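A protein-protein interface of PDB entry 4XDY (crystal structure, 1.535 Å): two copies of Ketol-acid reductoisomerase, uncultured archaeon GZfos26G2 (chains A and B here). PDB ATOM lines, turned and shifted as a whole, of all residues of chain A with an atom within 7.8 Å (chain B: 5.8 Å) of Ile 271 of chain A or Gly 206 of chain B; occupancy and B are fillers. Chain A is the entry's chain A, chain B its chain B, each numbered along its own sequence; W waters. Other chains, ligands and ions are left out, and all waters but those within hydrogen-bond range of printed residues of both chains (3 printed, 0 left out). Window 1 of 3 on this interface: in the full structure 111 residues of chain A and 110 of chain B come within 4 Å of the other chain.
Printed residues of chain B that touch a printed residue of chain A: Gln 200, Cys 201, Val 202, Leu 203, Cys 204, Gly 205, Gly 206, Leu 207, Val 208, Glu 209, Leu 210, Asn 213, Ile 271, Val 275 and Met 279. Hydrophobic or aromatic side chains of chain B that line the printed part of chain A: Val 202, Leu 203, Val 208, Leu 210, Ile 271, Val 275 and Met 279. Hydrophobic or aromatic side chains of chain A that line the printed part of chain B: Leu 210, Met 236, Met 263, Val 266, His 268, Ile 270, Ile 271 and Met 279. Among the printed residues, 30 pairs touch across the chains. Among the printed residues, no Asp or Glu carboxylate lies within 4 Å of a Lys or Arg side-chain nitrogen of the other chain.
The backbone NH (N) of Cys 204 of chain B sits at hydrogen-bond distance from the backbone carbonyl oxygen (O) of Glu 199 of chain B (3.0 Å). N of Gly 205 of chain B sits at hydrogen-bond distance from O of Glu 199 of chain B, at 3.0 Å. The backbone carbonyl oxygen of Gln 200 of chain B sits close to the backbone NH of Gly 205 of chain B, at 3.3 Å. The backbone NH (N) of Gly 206 of chain B sits at hydrogen-bond distance from the backbone carbonyl oxygen (O) of Gln 200 of chain B (3.4 Å). The backbone carbonyl oxygen (O) of Val 202 of chain B is in hydrogen-bond range of the backbone NH (N) of Leu 207 of chain B, at 3.0 Å. The backbone carbonyl oxygen (O) of Glu 209 of chain B lies within hydrogen-bond range of the side-chain amide nitrogen (ND2) of Asn 213 of chain B (2.8 Å).
C of Gly 206 of chain A touches CD2 of Leu 210 of chain B, 3.7 Å away. CD1 of Leu 210 of chain A touches O of Cys 201 of chain B, at 3.4 Å. Leu 210 of chain A touches Val 202 of chain B. Gly 205 of chain B touches Met 263 of chain A. CG2 of Val 266 of chain A touches OE1 of Gln 200 of chain B (3.6 Å). Gly 267 of chain A touches Glu 209 of chain B. O of Ile 270 of chain A touches CG2 of Val 275 of chain B (3.7 Å). Met 279 of chain B touches Ile 270 of chain A. Ile 271 of chain A touches Asn 213 of chain B. Asn 213 of chain B touches Lys 276 of chain A (OD1 to CB, 3.3 Å).
Water W1 bridges O of Ile 271 of chain B and OE1 of Glu 209 of chain A. Water W3 lies within hydrogen-bond range of the side-chain carboxylate (OE1) of Glu 209 of chain B (2.6 Å), the backbone carbonyl oxygen (O) of Ile 271 of chain A (2.7 Å) and the side-chain amide nitrogen (ND2) of Asn 213 of chain B (3.0 Å). Water W2 lies within hydrogen-bond range of O of Met 263 of chain A (2.7 Å), N of His 268 of chain A (2.8 Å) and OE2 of Glu 209 of chain B (2.8 Å).
Gly 206 of chain A touches Ile 271 of chain B, and with the chains exchanged Ile 271 of chain A touches Gly 206 of chain B. Glu 209 of chain A touches Ile 271 of chain B, and with the chains exchanged Ile 271 of chain A touches Glu 209 of chain B. Leu 210 of chain A touches Met 279 of chain B, and with the chains exchanged Met 279 of chain A touches Leu 210 of chain B. Ile 271 of chain A touches its own counterpart, Ile 271 of chain B. 6 positions are printed for both chains. Of the 30 pairs that touch across the chains among the printed residues, 9 have their exchanged pair printed and touching as well.
Of the printed residues of chain B, Leu 210 of chain A touches Cys 201, Val 202, Gly 206, Leu 207, Ile 271 and Met 279. Of the printed residues of chain B, Gly 262 of chain A touches Gln 200. Of chain B, only Gly 206 (3.9 Å), Glu 209 (3.7 Å), Asn 213 (3.9 Å) and Ile 271 (3.6 Å) come within 4 Å of Ile 271 of chain A. Of the printed residues of chain A, Leu 203 of chain B touches Met 236 (3.4 Å). Gly 206 of chain B touches just these residues of chain A: Leu 210 (3.8 Å) and Ile 271 (3.9 Å). The nearest residue of chain B that does not touch Ile 271 of chain A is Leu 210 of chain B (4.02 Å). The nearest printed residue of chain A that does not touch Glu 209 of chain B is Met 263 of chain A (4.8 Å).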
ATOM      1  N   GLY A 206      17.169 -21.404  33.284  1.00  0.00           N
ATOM      2  CA  GLY A 206      17.112 -20.081  32.676  1.00  0.00           C
ATOM      3  C   GLY A 206      16.257 -19.984  31.455  1.00  0.00           C
ATOM      4  O   GLY A 206      15.362 -19.132  31.392  1.00  0.00           O
ATOM      5  N   GLU A 209      12.365 -20.528  32.274  1.00  0.00           N
ATOM      6  CA  GLU A 209      11.833 -19.363  33.002  1.00  0.00           C
ATOM      7  C   GLU A 209      11.793 -18.125  32.134  1.00  0.00           C
ATOM      8  O   GLU A 209      10.836 -17.353  32.230  1.00  0.00           O
ATOM      9  CB  GLU A 209      12.585 -19.116  34.286  1.00  0.00           C
ATOM     10  CG  GLU A 209      12.463 -20.292  35.229  1.00  0.00           C
ATOM     11  CD  GLU A 209      11.043 -20.493  35.850  1.00  0.00           C
ATOM     12  OE1 GLU A 209      10.163 -19.612  35.666  1.00  0.00           O
ATOM     13  OE2 GLU A 209      10.836 -21.534  36.515  1.00  0.00           O
ATOM     14  N   LEU A 210      12.766 -18.000  31.212  1.00  0.00           N
ATOM     15  CA  LEU A 210      12.712 -16.897  30.257  1.00  0.00           C
ATOM     16  C   LEU A 210      11.481 -17.010  29.323  1.00  0.00           C
ATOM     17  O   LEU A 210      10.676 -16.033  29.215  1.00  0.00           O
ATOM     18  CB  LEU A 210      13.979 -16.772  29.462  1.00  0.00           C
ATOM     19  CG  LEU A 210      14.031 -15.696  28.380  1.00  0.00           C
ATOM     20  CD1 LEU A 210      14.096 -14.321  28.957  1.00  0.00           C
ATOM     21  CD2 LEU A 210      15.197 -15.967  27.465  1.00  0.00           C
ATOM     22  N   MET A 236      11.943 -19.577  19.149  1.00  0.00           N
ATOM     23  CA  MET A 236      13.227 -19.651  19.850  1.00  0.00           C
ATOM     24  C   MET A 236      14.187 -20.626  19.208  1.00  0.00           C
ATOM     25  O   MET A 236      15.413 -20.365  19.099  1.00  0.00           O
ATOM     26  CB  MET A 236      12.997 -20.031  21.274  1.00  0.00           C
ATOM     27  CG  MET A 236      14.213 -20.081  22.183  1.00  0.00           C
ATOM     28  SD  MET A 236      14.949 -18.411  22.447  1.00  0.00           S
ATOM     29  CE  MET A 236      13.995 -17.958  23.844  1.00  0.00           C
ATOM     30  N   GLY A 262      16.562  -3.412  19.214  1.00  0.00           N
ATOM     31  CA  GLY A 262      15.848  -3.825  20.418  1.00  0.00           C
ATOM     32  C   GLY A 262      16.672  -4.734  21.278  1.00  0.00           C
ATOM     33  O   GLY A 262      16.629  -4.630  22.509  1.00  0.00           O
ATOM     34  N   MET A 263      17.329  -5.698  20.679  1.00  0.00           N
ATOM     35  CA  MET A 263      18.169  -6.630  21.403  1.00  0.00           C
ATOM     36  C   MET A 263      19.179  -5.899  22.348  1.00  0.00           C
ATOM     37  O   MET A 263      19.269  -6.218  23.534  1.00  0.00           O
ATOM     38  CB  MET A 263      18.893  -7.505  20.407  1.00  0.00           C
ATOM     39  CG  MET A 263      19.940  -8.448  20.991  1.00  0.00           C
ATOM     40  SD  MET A 263      20.666  -9.709  19.931  1.00  0.00           S
ATOM     41  CE  MET A 263      21.268  -8.698  18.591  1.00  0.00           C
ATOM     42  N   VAL A 266      17.162  -3.093  24.837  1.00  0.00           N
ATOM     43  CA  VAL A 266      16.259  -3.574  25.834  1.00  0.00           C
ATOM     44  C   VAL A 266      16.688  -4.885  26.526  1.00  0.00           C
ATOM     45  O   VAL A 266      16.339  -5.122  27.696  1.00  0.00           O
ATOM     46  CB  VAL A 266      14.836  -3.708  25.197  1.00  0.00           C
ATOM     47  CG1 VAL A 266      13.851  -4.215  26.215  1.00  0.00           C
ATOM     48  CG2 VAL A 266      14.382  -2.378  24.605  1.00  0.00           C
ATOM     49  N   GLY A 267      17.397  -5.751  25.827  1.00  0.00           N
ATOM     50  CA  GLY A 267      17.720  -7.064  26.397  1.00  0.00           C
ATOM     51  C   GLY A 267      18.300  -6.969  27.781  1.00  0.00           C
ATOM     52  O   GLY A 267      17.872  -7.694  28.690  1.00  0.00           O
ATOM     53  N   HIS A 268      19.331  -6.115  27.933  1.00  0.00           N
ATOM     54  CA  HIS A 268      20.029  -5.984  29.229  1.00  0.00           C
ATOM     55  C   HIS A 268      19.154  -5.310  30.317  1.00  0.00           C
ATOM     56  O   HIS A 268      19.515  -5.372  31.493  1.00  0.00           O
ATOM     57  CB  HIS A 268      21.363  -5.252  29.060  1.00  0.00           C
ATOM     58  CG  HIS A 268      21.196  -3.818  28.735  1.00  0.00           C
ATOM     59  ND1 HIS A 268      20.959  -3.380  27.467  1.00  0.00           N
ATOM     60  CD2 HIS A 268      21.042  -2.739  29.544  1.00  0.00           C
ATOM     61  CE1 HIS A 268      20.801  -2.069  27.470  1.00  0.00           C
ATOM     62  NE2 HIS A 268      20.846  -1.656  28.718  1.00  0.00           N
ATOM     63  N   GLN A 269      18.067  -4.636  29.948  1.00  0.00           N
ATOM     64  CA  GLN A 269      17.093  -4.159  30.914  1.00  0.00           C
ATOM     65  C   GLN A 269      16.246  -5.270  31.479  1.00  0.00           C
ATOM     66  O   GLN A 269      15.690  -5.178  32.557  1.00  0.00           O
ATOM     67  CB  GLN A 269      16.213  -3.087  30.320  1.00  0.00           C
ATOM     68  CG  GLN A 269      16.960  -1.892  29.828  1.00  0.00           C
ATOM     69  CD  GLN A 269      16.002  -0.818  29.324  1.00  0.00           C
ATOM     70  OE1 GLN A 269      15.965  -0.463  28.153  1.00  0.00           O
ATOM     71  NE2 GLN A 269      15.228  -0.305  30.219  1.00  0.00           N
ATOM     72  N   ILE A 270      16.119  -6.352  30.732  1.00  0.00           N
ATOM     73  CA  ILE A 270      15.336  -7.510  31.199  1.00  0.00           C
ATOM     74  C   ILE A 270      16.223  -8.428  32.026  1.00  0.00           C
ATOM     75  O   ILE A 270      15.855  -8.826  33.094  1.00  0.00           O
ATOM     76  CB  ILE A 270      14.774  -8.268  29.916  1.00  0.00           C
ATOM     77  CG1 ILE A 270      13.934  -7.288  29.077  1.00  0.00           C
ATOM     78  CG2 ILE A 270      13.999  -9.491  30.388  1.00  0.00           C
ATOM     79  CD1 ILE A 270      12.851  -6.518  29.844  1.00  0.00           C
ATOM     80  N   ILE A 271      17.355  -8.805  31.445  1.00  0.00           N
ATOM     81  CA  ILE A 271      18.365  -9.722  32.012  1.00  0.00           C
ATOM     82  C   ILE A 271      19.620  -8.862  32.199  1.00  0.00           C
ATOM     83  O   ILE A 271      20.419  -8.676  31.255  1.00  0.00           O
ATOM     84  CB  ILE A 271      18.721 -10.883  31.084  1.00  0.00           C
ATOM     85  CG1 ILE A 271      17.491 -11.689  30.592  1.00  0.00           C
ATOM     86  CG2 ILE A 271      19.823 -11.750  31.694  1.00  0.00           C
ATOM     87  CD1 ILE A 271      16.635 -12.233  31.658  1.00  0.00           C
ATOM     88  N   GLY A 272      19.737  -8.371  33.428  1.00  0.00           N
ATOM     89  CA  GLY A 272      20.780  -7.423  33.785  1.00  0.00           C
ATOM     90  C   GLY A 272      21.708  -7.882  34.871  1.00  0.00           C
ATOM     91  O   GLY A 272      21.821  -9.073  35.148  1.00  0.00           O
ATOM     92  N   PRO A 273      22.419  -6.906  35.476  1.00  0.00           N
ATOM     93  CA  PRO A 273      23.393  -7.218  36.516  1.00  0.00           C
ATOM     94  C   PRO A 273      22.816  -7.985  37.655  1.00  0.00           C
ATOM     95  O   PRO A 273      23.544  -8.795  38.250  1.00  0.00           O
ATOM     96  CB  PRO A 273      23.875  -5.766  36.969  1.00  0.00           C
ATOM     97  CG  PRO A 273      23.740  -4.943  35.682  1.00  0.00           C
ATOM     98  CD  PRO A 273      22.471  -5.465  35.060  1.00  0.00           C
ATOM     99  N   GLU A 274      21.542  -7.765  38.020  1.00  0.00           N
ATOM    100  CA  GLU A 274      20.918  -8.499  39.126  1.00  0.00           C
ATOM    101  C   GLU A 274      20.870  -9.986  38.810  1.00  0.00           C
ATOM    102  O   GLU A 274      21.107 -10.869  39.675  1.00  0.00           O
ATOM    103  CB  GLU A 274      19.482  -8.008  39.398  1.00  0.00           C
ATOM    104  CG  GLU A 274      19.434  -6.527  39.704  1.00  0.00           C
ATOM    105  CD  GLU A 274      19.492  -5.512  38.493  1.00  0.00           C
ATOM    106  OE1 GLU A 274      19.707  -5.822  37.259  1.00  0.00           O
ATOM    107  OE2 GLU A 274      19.365  -4.306  38.815  1.00  0.00           O
ATOM    108  N   VAL A 275      20.561 -10.293  37.558  1.00  0.00           N
ATOM    109  CA  VAL A 275      20.581 -11.719  37.098  1.00  0.00           C
ATOM    110  C   VAL A 275      21.990 -12.345  37.176  1.00  0.00           C
ATOM    111  O   VAL A 275      22.175 -13.496  37.665  1.00  0.00           O
ATOM    112  CB  VAL A 275      20.017 -11.885  35.645  1.00  0.00           C
ATOM    113  CG1 VAL A 275      20.244 -13.334  35.140  1.00  0.00           C
ATOM    114  CG2 VAL A 275      18.537 -11.567  35.646  1.00  0.00           C
ATOM    115  N   LYS A 276      22.979 -11.588  36.796  1.00  0.00           N
ATOM    116  CA  LYS A 276      24.341 -12.077  36.847  1.00  0.00           C
ATOM    117  C   LYS A 276      24.749 -12.415  38.306  1.00  0.00           C
ATOM    118  O   LYS A 276      25.424 -13.444  38.569  1.00  0.00           O
ATOM    119  CB  LYS A 276      25.326 -11.105  36.221  1.00  0.00           C
ATOM    120  CG  LYS A 276      26.706 -11.685  36.024  1.00  0.00           C
ATOM    121  CD  LYS A 276      27.683 -10.724  35.313  1.00  0.00           C
ATOM    122  CE  LYS A 276      29.046 -11.292  35.147  1.00  0.00           C
ATOM    123  NZ  LYS A 276      29.872 -10.380  34.325  1.00  0.00           N
ATOM    124  N   MET A 279      23.213 -15.548  39.410  1.00  0.00           N
ATOM    125  CA  MET A 279      24.021 -16.640  38.795  1.00  0.00           C
ATOM    126  C   MET A 279      25.283 -16.957  39.588  1.00  0.00           C
ATOM    127  O   MET A 279      25.616 -18.118  39.809  1.00  0.00           O
ATOM    128  CB  MET A 279      24.384 -16.305  37.348  1.00  0.00           C
ATOM    129  CG  MET A 279      23.213 -16.349  36.388  1.00  0.00           C
ATOM    130  SD  MET A 279      23.847 -15.993  34.719  1.00  0.00           S
ATOM    131  CE  MET A 279      22.478 -16.465  33.637  1.00  0.00           C
ATOM    132  N   GLU B 199      11.102 -10.020  20.466  1.00  0.00           N
ATOM    133  CA  GLU B 199      12.465  -9.958  20.035  1.00  0.00           C
ATOM    134  C   GLU B 199      13.318  -9.282  21.100  1.00  0.00           C
ATOM    135  O   GLU B 199      14.465  -9.699  21.337  1.00  0.00           O
ATOM    136  CB  GLU B 199      12.622  -9.296  18.646  1.00  0.00           C
ATOM    137  CG  GLU B 199      12.204  -7.848  18.621  1.00  0.00           C
ATOM    138  CD  GLU B 199      11.794  -7.344  17.235  1.00  0.00           C
ATOM    139  OE1 GLU B 199      11.362  -8.181  16.379  1.00  0.00           O
ATOM    140  OE2 GLU B 199      11.806  -6.082  17.035  1.00  0.00           O
ATOM    141  N   GLN B 200      12.781  -8.305  21.782  1.00  0.00           N
ATOM    142  CA  GLN B 200      13.511  -7.548  22.755  1.00  0.00           C
ATOM    143  C   GLN B 200      13.764  -8.362  24.016  1.00  0.00           C
ATOM    144  O   GLN B 200      14.886  -8.390  24.511  1.00  0.00           O
ATOM    145  CB  GLN B 200      12.704  -6.329  23.190  1.00  0.00           C
ATOM    146  CG  GLN B 200      12.797  -5.185  22.161  1.00  0.00           C
ATOM    147  CD  GLN B 200      11.819  -4.059  22.349  1.00  0.00           C
ATOM    148  OE1 GLN B 200      11.295  -3.877  23.412  1.00  0.00           O
ATOM    149  NE2 GLN B 200      11.513  -3.331  21.281  1.00  0.00           N
ATOM    150  N   CYS B 201      12.697  -9.036  24.492  1.00  0.00           N
ATOM    151  CA  CYS B 201      12.658  -9.610  25.833  1.00  0.00           C
ATOM    152  C   CYS B 201      12.962 -11.091  25.917  1.00  0.00           C
ATOM    153  O   CYS B 201      13.292 -11.612  26.982  1.00  0.00           O
ATOM    154  CB  CYS B 201      11.342  -9.313  26.533  1.00  0.00           C
ATOM    155  SG  CYS B 201      11.041  -7.549  26.767  1.00  0.00           S
ATOM    156  N   VAL B 202      12.750 -11.803  24.803  1.00  0.00           N
ATOM    157  CA  VAL B 202      12.778 -13.245  24.809  1.00  0.00           C
ATOM    158  C   VAL B 202      13.759 -13.811  23.779  1.00  0.00           C
ATOM    159  O   VAL B 202      14.758 -14.432  24.147  1.00  0.00           O
ATOM    160  CB  VAL B 202      11.359 -13.879  24.675  1.00  0.00           C
ATOM    161  CG1 VAL B 202      11.407 -15.352  24.719  1.00  0.00           C
ATOM    162  CG2 VAL B 202      10.432 -13.409  25.755  1.00  0.00           C
ATOM    163  N   LEU B 203      13.472 -13.634  22.486  1.00  0.00           N
ATOM    164  CA  LEU B 203      14.153 -14.265  21.415  1.00  0.00           C
ATOM    165  C   LEU B 203      15.577 -13.746  21.177  1.00  0.00           C
ATOM    166  O   LEU B 203      16.491 -14.571  20.877  1.00  0.00           O
ATOM    167  CB  LEU B 203      13.363 -14.104  20.125  1.00  0.00           C
ATOM    168  CG  LEU B 203      11.978 -14.783  19.989  1.00  0.00           C
ATOM    169  CD1 LEU B 203      11.310 -14.332  18.693  1.00  0.00           C
ATOM    170  CD2 LEU B 203      12.136 -16.287  20.124  1.00  0.00           C
ATOM    171  N   CYS B 204      15.773 -12.420  21.232  1.00  0.00           N
ATOM    172  CA  CYS B 204      17.090 -11.800  20.878  1.00  0.00           C
ATOM    173  C   CYS B 204      17.716 -11.144  22.113  1.00  0.00           C
ATOM    174  O   CYS B 204      18.680 -11.642  22.610  1.00  0.00           O
ATOM    175  CB  CYS B 204      16.915 -10.820  19.719  1.00  0.00           C
ATOM    176  SG  CYS B 204      16.128 -11.563  18.283  1.00  0.00           S
ATOM    177  N   GLY B 205      17.079 -10.143  22.714  1.00  0.00           N
ATOM    178  CA  GLY B 205      17.566  -9.516  23.905  1.00  0.00           C
ATOM    179  C   GLY B 205      17.703 -10.461  25.070  1.00  0.00           C
ATOM    180  O   GLY B 205      18.771 -10.586  25.680  1.00  0.00           O
ATOM    181  N   GLY B 206      16.612 -11.170  25.349  1.00  0.00           N
ATOM    182  CA  GLY B 206      16.570 -12.089  26.480  1.00  0.00           C
ATOM    183  C   GLY B 206      17.566 -13.261  26.318  1.00  0.00           C
ATOM    184  O   GLY B 206      18.415 -13.511  27.230  1.00  0.00           O
ATOM    185  N   LEU B 207      17.501 -13.909  25.183  1.00  0.00           N
ATOM    186  CA  LEU B 207      18.336 -15.079  24.914  1.00  0.00           C
ATOM    187  C   LEU B 207      19.812 -14.718  24.986  1.00  0.00           C
ATOM    188  O   LEU B 207      20.623 -15.421  25.655  1.00  0.00           O
ATOM    189  CB  LEU B 207      17.994 -15.635  23.535  1.00  0.00           C
ATOM    190  CG  LEU B 207      18.944 -16.675  22.978  1.00  0.00           C
ATOM    191  CD1 LEU B 207      18.839 -17.942  23.795  1.00  0.00           C
ATOM    192  CD2 LEU B 207      18.778 -16.882  21.478  1.00  0.00           C
ATOM    193  N   VAL B 208      20.182 -13.641  24.287  1.00  0.00           N
ATOM    194  CA  VAL B 208      21.607 -13.293  24.202  1.00  0.00           C
ATOM    195  C   VAL B 208      22.181 -12.878  25.522  1.00  0.00           C
ATOM    196  O   VAL B 208      23.276 -13.273  25.902  1.00  0.00           O
ATOM    197  CB  VAL B 208      21.896 -12.298  23.049  1.00  0.00           C
ATOM    198  CG1 VAL B 208      23.304 -11.768  23.112  1.00  0.00           C
ATOM    199  CG2 VAL B 208      21.649 -13.003  21.703  1.00  0.00           C
ATOM    200  N   GLU B 209      21.434 -12.070  26.283  1.00  0.00           N
ATOM    201  CA  GLU B 209      21.855 -11.656  27.595  1.00  0.00           C
ATOM    202  C   GLU B 209      21.890 -12.824  28.573  1.00  0.00           C
ATOM    203  O   GLU B 209      22.803 -12.877  29.415  1.00  0.00           O
ATOM    204  CB  GLU B 209      20.995 -10.537  28.125  1.00  0.00           C
ATOM    205  CG  GLU B 209      21.139  -9.255  27.277  1.00  0.00           C
ATOM    206  CD  GLU B 209      22.543  -8.584  27.333  1.00  0.00           C
ATOM    207  OE1 GLU B 209      23.296  -8.907  28.248  1.00  0.00           O
ATOM    208  OE2 GLU B 209      22.779  -7.651  26.493  1.00  0.00           O
ATOM    209  N   LEU B 210      20.982 -13.786  28.426  1.00  0.00           N
ATOM    210  CA  LEU B 210      21.031 -14.962  29.300  1.00  0.00           C
ATOM    211  C   LEU B 210      22.334 -15.741  29.033  1.00  0.00           C
ATOM    212  O   LEU B 210      23.050 -16.119  30.000  1.00  0.00           O
ATOM    213  CB  LEU B 210      19.807 -15.848  29.087  1.00  0.00           C
ATOM    214  CG  LEU B 210      19.768 -17.129  29.855  1.00  0.00           C
ATOM    215  CD1 LEU B 210      19.526 -16.890  31.345  1.00  0.00           C
ATOM    216  CD2 LEU B 210      18.624 -17.995  29.339  1.00  0.00           C
ATOM    217  N   MET B 211      22.600 -16.060  27.778  1.00  0.00           N
ATOM    218  CA  MET B 211      23.779 -16.859  27.457  1.00  0.00           C
ATOM    219  C   MET B 211      25.066 -16.109  27.804  1.00  0.00           C
ATOM    220  O   MET B 211      26.008 -16.735  28.333  1.00  0.00           O
ATOM    221  CB  MET B 211      23.798 -17.267  26.005  1.00  0.00           C
ATOM    222  CG  MET B 211      22.771 -18.293  25.650  1.00  0.00           C
ATOM    223  SD  MET B 211      22.850 -18.843  23.941  1.00  0.00           S
ATOM    224  CE  MET B 211      22.775 -17.319  23.064  1.00  0.00           C
ATOM    225  N   ASN B 213      25.626 -13.651  30.062  1.00  0.00           N
ATOM    226  CA  ASN B 213      25.805 -13.582  31.496  1.00  0.00           C
ATOM    227  C   ASN B 213      26.266 -14.893  32.095  1.00  0.00           C
ATOM    228  O   ASN B 213      27.207 -14.949  32.864  1.00  0.00           O
ATOM    229  CB  ASN B 213      24.567 -13.040  32.266  1.00  0.00           C
ATOM    230  CG  ASN B 213      24.483 -11.540  32.196  1.00  0.00           C
ATOM    231  OD1 ASN B 213      25.202 -10.823  32.912  1.00  0.00           O
ATOM    232  ND2 ASN B 213      23.637 -11.026  31.332  1.00  0.00           N
ATOM    233  N   ILE B 271      15.847 -16.162  37.077  1.00  0.00           N
ATOM    234  CA  ILE B 271      14.890 -15.408  36.254  1.00  0.00           C
ATOM    235  C   ILE B 271      13.611 -15.417  37.071  1.00  0.00           C
ATOM    236  O   ILE B 271      12.838 -16.352  37.009  1.00  0.00           O
ATOM    237  CB  ILE B 271      14.595 -16.097  34.900  1.00  0.00           C
ATOM    238  CG1 ILE B 271      15.870 -16.355  34.072  1.00  0.00           C
ATOM    239  CG2 ILE B 271      13.558 -15.344  34.042  1.00  0.00           C
ATOM    240  CD1 ILE B 271      16.678 -15.167  33.810  1.00  0.00           C
ATOM    241  N   VAL B 275      12.498  -9.956  36.767  1.00  0.00           N
ATOM    242  CA  VAL B 275      12.508 -10.055  35.300  1.00  0.00           C
ATOM    243  C   VAL B 275      11.133  -9.883  34.693  1.00  0.00           C
ATOM    244  O   VAL B 275      10.980  -9.172  33.656  1.00  0.00           O
ATOM    245  CB  VAL B 275      13.118 -11.410  34.790  1.00  0.00           C
ATOM    246  CG1 VAL B 275      12.975 -11.509  33.307  1.00  0.00           C
ATOM    247  CG2 VAL B 275      14.548 -11.458  35.262  1.00  0.00           C
ATOM    248  N   MET B 279       9.887  -7.089  32.064  1.00  0.00           N
ATOM    249  CA  MET B 279       9.210  -7.450  30.802  1.00  0.00           C
ATOM    250  C   MET B 279       7.933  -6.610  30.649  1.00  0.00           C
ATOM    251  O   MET B 279       7.657  -6.093  29.559  1.00  0.00           O
ATOM    252  CB  MET B 279       8.907  -8.930  30.792  1.00  0.00           C
ATOM    253  CG  MET B 279      10.117  -9.780  30.428  1.00  0.00           C
ATOM    254  SD  MET B 279       9.619 -11.526  30.450  1.00  0.00           S
ATOM    255  CE  MET B 279      11.148 -12.351  29.992  1.00  0.00           C
HETATM  256  O   HOH W   1      10.377 -17.060  37.201  1.00  0.00           O
HETATM  257  O   HOH W   2      20.895  -5.771  25.677  1.00  0.00           O
HETATM  258  O   HOH W   3      22.977  -8.169  30.745  1.00  0.00           O
